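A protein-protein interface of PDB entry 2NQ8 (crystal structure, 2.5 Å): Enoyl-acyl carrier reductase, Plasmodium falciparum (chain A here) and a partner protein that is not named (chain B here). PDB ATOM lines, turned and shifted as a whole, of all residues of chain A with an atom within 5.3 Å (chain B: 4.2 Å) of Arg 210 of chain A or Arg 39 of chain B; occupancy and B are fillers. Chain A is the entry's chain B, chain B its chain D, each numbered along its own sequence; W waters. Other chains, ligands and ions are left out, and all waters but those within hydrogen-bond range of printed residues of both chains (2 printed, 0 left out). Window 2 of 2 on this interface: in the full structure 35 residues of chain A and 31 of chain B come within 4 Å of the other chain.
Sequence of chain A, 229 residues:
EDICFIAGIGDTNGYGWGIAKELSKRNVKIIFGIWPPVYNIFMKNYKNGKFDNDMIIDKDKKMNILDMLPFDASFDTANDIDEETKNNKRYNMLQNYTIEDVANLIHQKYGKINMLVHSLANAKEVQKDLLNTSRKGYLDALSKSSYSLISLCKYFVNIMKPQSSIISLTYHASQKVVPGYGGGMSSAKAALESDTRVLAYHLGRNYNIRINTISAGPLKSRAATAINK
The guanidinium group (NH2) of Arg 210 of chain A sits at hydrogen-bond distance from the backbone carbonyl oxygen (O) of Leu 33 of chain B.
The side-chain hydroxyl (OG) of Ser 165 of chain A lies within hydrogen-bond range of the backbone carbonyl oxygen (O) of Leu 33 of chain B.
NH2 of Arg 210 of chain A sits at hydrogen-bond distance from O of Ser 35 of chain B.
The side-chain hydroxyl of Ser 38 of chain B lies within hydrogen-bond range of the guanidinium group of Arg 210 of chain A, 2.9 Å away.
NH1 of Arg 36 of chain B lies close to NE2 of Gln 163 of chain A (2.8 Å).
The backbone NH (N) of Thr 42 of chain B sits close to the side-chain amide oxygen (OD1) of Asn 212 of chain A (3.5 Å).
NH1 of Arg 210 of chain A sits at hydrogen-bond distance from O of Ile 41 of chain B, 3.0 Å away.
OG1 of Thr 42 of chain B is in hydrogen-bond range of N of Ile 211 of chain A (3.4 Å).
The backbone carbonyl oxygen (O) of Ile 41 of chain B lies within hydrogen-bond range of the side-chain amide nitrogen (ND2) of Asn 212 of chain A (3.2 Å).
N of Gln 163 of chain A is in hydrogen-bond range of O of Asn 208 of chain A (2.9 Å).
N of Asn 212 of chain A sits at hydrogen-bond distance from O of Ile 166 of chain A (3.1 Å).
OG of Ser 38 of chain B is in hydrogen-bond range of O of Leu 33 of chain B (2.8 Å).
The side-chain hydroxyl of Ser 35 of chain B lies close to the backbone NH of Glu 37 of chain B (3.2 Å).
The backbone carbonyl oxygen of Ser 35 of chain B sits at hydrogen-bond distance from the side-chain hydroxyl of Ser 38 of chain B.
O of Arg 210 of chain A is in hydrogen-bond range of N of Ile 166 of chain A (2.8 Å).
Arg 210 of chain A touches Arg 39 of chain B.
Arg 210 of chain A touches Thr 42 of chain B.
Of the printed residues of chain B, Ser 165 of chain A touches Leu 33.
Printed residues of chain B within 4 Å of Arg 210 of chain A: Leu 33 (2.9 Å), Ser 35 (2.9 Å), Ser 38 (2.9 Å), Arg 39 (3.2 Å), Ile 41 (3.0 Å) and Thr 42 (3.7 Å).
Printed residues of chain B within 4 Å of Asn 212 of chain A: Ile 41 (3.2 Å) and Thr 42 (3.2 Å).
Of the printed residues of chain A, Leu 33 of chain B touches Ser 165 (2.9 Å) and Arg 210 (2.9 Å).
Of the printed residues of chain A, Arg 36 of chain B touches Gln 163 (2.8 Å).
Arg 39 of chain B touches just one residue of chain A: Arg 210.
The nearest printed residue of chain B that does not touch Arg 210 of chain A is Ala 40 of chain B (4.5 Å).
The nearest residue of chain A that does not touch Arg 39 of chain B is Gln 163 of chain A (4.9 Å).
The nearest printed residue of chain A that does not touch Ser 35 of chain B is Ser 165 of chain A (5.1 Å).
Of the 9 printed residues of chain A, 5 touch a printed residue of chain B.
Printed residues of chain A that touch a printed residue of chain B: Gln 163, Ser 165, Arg 210, Ile 211 and Asn 212.
Printed residues of chain B that touch a printed residue of chain A: Leu 33, Ser 35, Arg 36, Ser 38, Arg 39, Ile 41 and Thr 42.
Hydrophobic or aromatic side chains of chain B that line the printed part of chain A: Ile 41.
Along chain B the printed residues that touch a printed residue of chain A span positions 33 to 42.
Water W1 bridges OG1 of Thr 42 of chain B and O of Ile 209 of chain A.
Water W2 lies within hydrogen-bond range of O of Ile 166 of chain A (2.6 Å), OG of Ser 165 of chain A (2.7 Å), ND2 of Asn 212 of chain A (3.0 Å) and O of Leu 33 of chain B (3.5 Å).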
ATOM      1  N   GLN A 163       5.033  26.745 -28.028  1.00  0.00           N
ATOM      2  CA  GLN A 163       3.610  27.072 -28.023  1.00  0.00           C
ATOM      3  C   GLN A 163       2.796  26.252 -29.007  1.00  0.00           C
ATOM      4  O   GLN A 163       1.618  26.524 -29.221  1.00  0.00           O
ATOM      5  CB  GLN A 163       3.394  28.567 -28.296  1.00  0.00           C
ATOM      6  CG  GLN A 163       4.116  29.470 -27.300  1.00  0.00           C
ATOM      7  CD  GLN A 163       3.738  30.931 -27.436  1.00  0.00           C
ATOM      8  OE1 GLN A 163       3.827  31.513 -28.515  1.00  0.00           O
ATOM      9  NE2 GLN A 163       3.314  31.534 -26.332  1.00  0.00           N
ATOM     10  N   SER A 164       3.423  25.251 -29.613  1.00  0.00           N
ATOM     11  CA  SER A 164       2.709  24.391 -30.548  1.00  0.00           C
ATOM     12  C   SER A 164       1.806  23.467 -29.736  1.00  0.00           C
ATOM     13  O   SER A 164       2.018  23.275 -28.540  1.00  0.00           O
ATOM     14  CB  SER A 164       3.692  23.574 -31.385  1.00  0.00           C
ATOM     15  OG  SER A 164       4.552  24.426 -32.121  1.00  0.00           O
ATOM     16  N   SER A 165       0.810  22.884 -30.389  1.00  0.00           N
ATOM     17  CA  SER A 165      -0.141  22.015 -29.710  1.00  0.00           C
ATOM     18  C   SER A 165      -0.260  20.632 -30.342  1.00  0.00           C
ATOM     19  O   SER A 165      -0.111  20.470 -31.553  1.00  0.00           O
ATOM     20  CB  SER A 165      -1.512  22.706 -29.686  1.00  0.00           C
ATOM     21  OG  SER A 165      -2.504  21.890 -29.096  1.00  0.00           O
ATOM     22  N   ILE A 166      -0.537  19.640 -29.501  1.00  0.00           N
ATOM     23  CA  ILE A 166      -0.684  18.254 -29.932  1.00  0.00           C
ATOM     24  C   ILE A 166      -2.019  17.719 -29.398  1.00  0.00           C
ATOM     25  O   ILE A 166      -2.462  18.109 -28.321  1.00  0.00           O
ATOM     26  CB  ILE A 166       0.445  17.346 -29.338  1.00  0.00           C
ATOM     27  CG1 ILE A 166       1.824  17.865 -29.733  1.00  0.00           C
ATOM     28  CG2 ILE A 166       0.267  15.893 -29.821  1.00  0.00           C
ATOM     29  CD1 ILE A 166       2.952  17.080 -29.121  1.00  0.00           C
ATOM     30  N   ASN A 208       7.336  24.071 -23.651  1.00  0.00           N
ATOM     31  CA  ASN A 208       6.204  24.982 -23.664  1.00  0.00           C
ATOM     32  C   ASN A 208       5.241  24.536 -24.776  1.00  0.00           C
ATOM     33  O   ASN A 208       4.701  25.352 -25.526  1.00  0.00           O
ATOM     34  CB  ASN A 208       6.685  26.418 -23.907  1.00  0.00           C
ATOM     35  CG  ASN A 208       5.590  27.443 -23.699  1.00  0.00           C
ATOM     36  OD1 ASN A 208       4.856  27.390 -22.711  1.00  0.00           O
ATOM     37  ND2 ASN A 208       5.478  28.390 -24.622  1.00  0.00           N
ATOM     38  N   ILE A 209       5.051  23.223 -24.887  1.00  0.00           N
ATOM     39  CA  ILE A 209       4.148  22.648 -25.878  1.00  0.00           C
ATOM     40  C   ILE A 209       3.016  21.949 -25.135  1.00  0.00           C
ATOM     41  O   ILE A 209       3.235  21.314 -24.097  1.00  0.00           O
ATOM     42  CB  ILE A 209       4.878  21.628 -26.780  1.00  0.00           C
ATOM     43  CG1 ILE A 209       5.845  22.367 -27.716  1.00  0.00           C
ATOM     44  CG2 ILE A 209       3.862  20.805 -27.579  1.00  0.00           C
ATOM     45  CD1 ILE A 209       6.773  21.454 -28.491  1.00  0.00           C
ATOM     46  N   ARG A 210       1.807  22.072 -25.667  1.00  0.00           N
ATOM     47  CA  ARG A 210       0.640  21.463 -25.046  1.00  0.00           C
ATOM     48  C   ARG A 210       0.201  20.172 -25.729  1.00  0.00           C
ATOM     49  O   ARG A 210       0.429  19.971 -26.928  1.00  0.00           O
ATOM     50  CB  ARG A 210      -0.529  22.453 -25.053  1.00  0.00           C
ATOM     51  CG  ARG A 210      -0.223  23.758 -24.361  1.00  0.00           C
ATOM     52  CD  ARG A 210      -1.451  24.633 -24.263  1.00  0.00           C
ATOM     53  NE  ARG A 210      -1.915  25.122 -25.558  1.00  0.00           N
ATOM     54  CZ  ARG A 210      -3.017  24.702 -26.182  1.00  0.00           C
ATOM     55  NH1 ARG A 210      -3.784  23.765 -25.634  1.00  0.00           N
ATOM     56  NH2 ARG A 210      -3.366  25.245 -27.347  1.00  0.00           N
ATOM     57  N   ILE A 211      -0.430  19.300 -24.949  1.00  0.00           N
ATOM     58  CA  ILE A 211      -0.947  18.044 -25.465  1.00  0.00           C
ATOM     59  C   ILE A 211      -2.208  17.691 -24.693  1.00  0.00           C
ATOM     60  O   ILE A 211      -2.225  17.718 -23.464  1.00  0.00           O
ATOM     61  CB  ILE A 211       0.082  16.896 -25.343  1.00  0.00           C
ATOM     62  CG1 ILE A 211      -0.521  15.601 -25.902  1.00  0.00           C
ATOM     63  CG2 ILE A 211       0.522  16.728 -23.899  1.00  0.00           C
ATOM     64  CD1 ILE A 211       0.485  14.465 -26.030  1.00  0.00           C
ATOM     65  N   ASN A 212      -3.273  17.401 -25.433  1.00  0.00           N
ATOM     66  CA  ASN A 212      -4.559  17.044 -24.858  1.00  0.00           C
ATOM     67  C   ASN A 212      -5.143  15.903 -25.664  1.00  0.00           C
ATOM     68  O   ASN A 212      -4.652  15.573 -26.748  1.00  0.00           O
ATOM     69  CB  ASN A 212      -5.527  18.224 -24.924  1.00  0.00           C
ATOM     70  CG  ASN A 212      -5.164  19.338 -23.964  1.00  0.00           C
ATOM     71  OD1 ASN A 212      -5.458  19.267 -22.768  1.00  0.00           O
ATOM     72  ND2 ASN A 212      -4.514  20.374 -24.482  1.00  0.00           N
ATOM     73  N   LEU B  33      -8.450  23.241 -29.511  1.00  0.00           N
ATOM     74  CA  LEU B  33      -7.371  22.778 -28.657  1.00  0.00           C
ATOM     75  C   LEU B  33      -6.005  23.018 -29.292  1.00  0.00           C
ATOM     76  O   LEU B  33      -5.009  23.203 -28.595  1.00  0.00           O
ATOM     77  CB  LEU B  33      -7.547  21.288 -28.360  1.00  0.00           C
ATOM     78  CG  LEU B  33      -8.683  20.945 -27.400  1.00  0.00           C
ATOM     79  CD1 LEU B  33      -8.991  19.446 -27.459  1.00  0.00           C
ATOM     80  CD2 LEU B  33      -8.284  21.378 -25.994  1.00  0.00           C
ATOM     81  N   SER B  35      -5.356  25.556 -31.391  1.00  0.00           N
ATOM     82  CA  SER B  35      -5.121  26.993 -31.489  1.00  0.00           C
ATOM     83  C   SER B  35      -4.691  27.590 -30.139  1.00  0.00           C
ATOM     84  O   SER B  35      -4.861  26.970 -29.086  1.00  0.00           O
ATOM     85  CB  SER B  35      -6.384  27.706 -31.990  1.00  0.00           C
ATOM     86  OG  SER B  35      -7.296  27.958 -30.930  1.00  0.00           O
ATOM     87  N   ARG B  36      -4.133  28.797 -30.190  1.00  0.00           N
ATOM     88  CA  ARG B  36      -3.674  29.519 -29.005  1.00  0.00           C
ATOM     89  C   ARG B  36      -4.817  29.829 -28.039  1.00  0.00           C
ATOM     90  O   ARG B  36      -4.591  30.112 -26.861  1.00  0.00           O
ATOM     91  CB  ARG B  36      -2.987  30.823 -29.432  1.00  0.00           C
ATOM     92  CG  ARG B  36      -1.548  30.645 -29.874  1.00  0.00           C
ATOM     93  CD  ARG B  36      -0.630  30.606 -28.662  1.00  0.00           C
ATOM     94  NE  ARG B  36      -0.609  31.908 -27.993  1.00  0.00           N
ATOM     95  CZ  ARG B  36      -0.063  32.139 -26.803  1.00  0.00           C
ATOM     96  NH1 ARG B  36       0.509  31.147 -26.129  1.00  0.00           N
ATOM     97  NH2 ARG B  36      -0.081  33.369 -26.294  1.00  0.00           N
ATOM     98  N   GLU B  37      -6.043  29.771 -28.545  1.00  0.00           N
ATOM     99  CA  GLU B  37      -7.215  30.032 -27.724  1.00  0.00           C
ATOM    100  C   GLU B  37      -7.275  29.134 -26.485  1.00  0.00           C
ATOM    101  O   GLU B  37      -7.928  29.474 -25.500  1.00  0.00           O
ATOM    102  CB  GLU B  37      -8.488  29.827 -28.542  1.00  0.00           C
ATOM    103  CG  GLU B  37      -8.713  30.859 -29.621  1.00  0.00           C
ATOM    104  CD  GLU B  37      -8.670  32.262 -29.075  1.00  0.00           C
ATOM    105  OE1 GLU B  37      -7.625  32.924 -29.242  1.00  0.00           O
ATOM    106  OE2 GLU B  37      -9.674  32.697 -28.466  1.00  0.00           O
ATOM    107  N   SER B  38      -6.602  27.992 -26.541  1.00  0.00           N
ATOM    108  CA  SER B  38      -6.592  27.056 -25.426  1.00  0.00           C
ATOM    109  C   SER B  38      -5.215  26.975 -24.767  1.00  0.00           C
ATOM    110  O   SER B  38      -4.901  25.992 -24.081  1.00  0.00           O
ATOM    111  CB  SER B  38      -7.023  25.666 -25.911  1.00  0.00           C
ATOM    112  OG  SER B  38      -6.227  25.214 -26.995  1.00  0.00           O
ATOM    113  N   ARG B  39      -4.407  28.017 -24.970  1.00  0.00           N
ATOM    114  CA  ARG B  39      -3.051  28.080 -24.416  1.00  0.00           C
ATOM    115  C   ARG B  39      -2.935  27.669 -22.944  1.00  0.00           C
ATOM    116  O   ARG B  39      -1.851  27.290 -22.495  1.00  0.00           O
ATOM    117  CB  ARG B  39      -2.472  29.492 -24.581  1.00  0.00           C
ATOM    118  CG  ARG B  39      -3.113  30.535 -23.671  1.00  0.00           C
ATOM    119  CD  ARG B  39      -2.599  31.943 -23.973  1.00  0.00           C
ATOM    120  NE  ARG B  39      -1.183  32.121 -23.655  1.00  0.00           N
ATOM    121  CZ  ARG B  39      -0.719  32.853 -22.644  1.00  0.00           C
ATOM    122  NH1 ARG B  39      -1.555  33.490 -21.830  1.00  0.00           N
ATOM    123  NH2 ARG B  39       0.591  32.963 -22.456  1.00  0.00           N
ATOM    124  N   ALA B  40      -4.034  27.740 -22.195  1.00  0.00           N
ATOM    125  CA  ALA B  40      -4.003  27.373 -20.778  1.00  0.00           C
ATOM    126  C   ALA B  40      -4.508  25.959 -20.461  1.00  0.00           C
ATOM    127  O   ALA B  40      -4.529  25.557 -19.292  1.00  0.00           O
ATOM    128  CB  ALA B  40      -4.783  28.404 -19.948  1.00  0.00           C
ATOM    129  N   ILE B  41      -4.903  25.209 -21.489  1.00  0.00           N
ATOM    130  CA  ILE B  41      -5.395  23.842 -21.293  1.00  0.00           C
ATOM    131  C   ILE B  41      -4.334  22.830 -21.697  1.00  0.00           C
ATOM    132  O   ILE B  41      -3.744  22.951 -22.773  1.00  0.00           O
ATOM    133  CB  ILE B  41      -6.646  23.546 -22.157  1.00  0.00           C
ATOM    134  CG1 ILE B  41      -7.727  24.615 -21.928  1.00  0.00           C
ATOM    135  CG2 ILE B  41      -7.204  22.172 -21.801  1.00  0.00           C
ATOM    136  CD1 ILE B  41      -8.970  24.419 -22.787  1.00  0.00           C
ATOM    137  N   THR B  42      -4.087  21.831 -20.852  1.00  0.00           N
ATOM    138  CA  THR B  42      -3.105  20.803 -21.189  1.00  0.00           C
ATOM    139  C   THR B  42      -3.227  19.546 -20.319  1.00  0.00           C
ATOM    140  O   THR B  42      -3.648  19.618 -19.160  1.00  0.00           O
ATOM    141  CB  THR B  42      -1.656  21.363 -21.096  1.00  0.00           C
ATOM    142  OG1 THR B  42      -0.754  20.468 -21.760  1.00  0.00           O
ATOM    143  CG2 THR B  42      -1.221  21.519 -19.632  1.00  0.00           C
HETATM  144  O   HOH W   1       1.745  20.691 -21.489  1.00  0.00           O
HETATM  145  O   HOH W   2      -3.742  20.206 -27.404  1.00  0.00           O
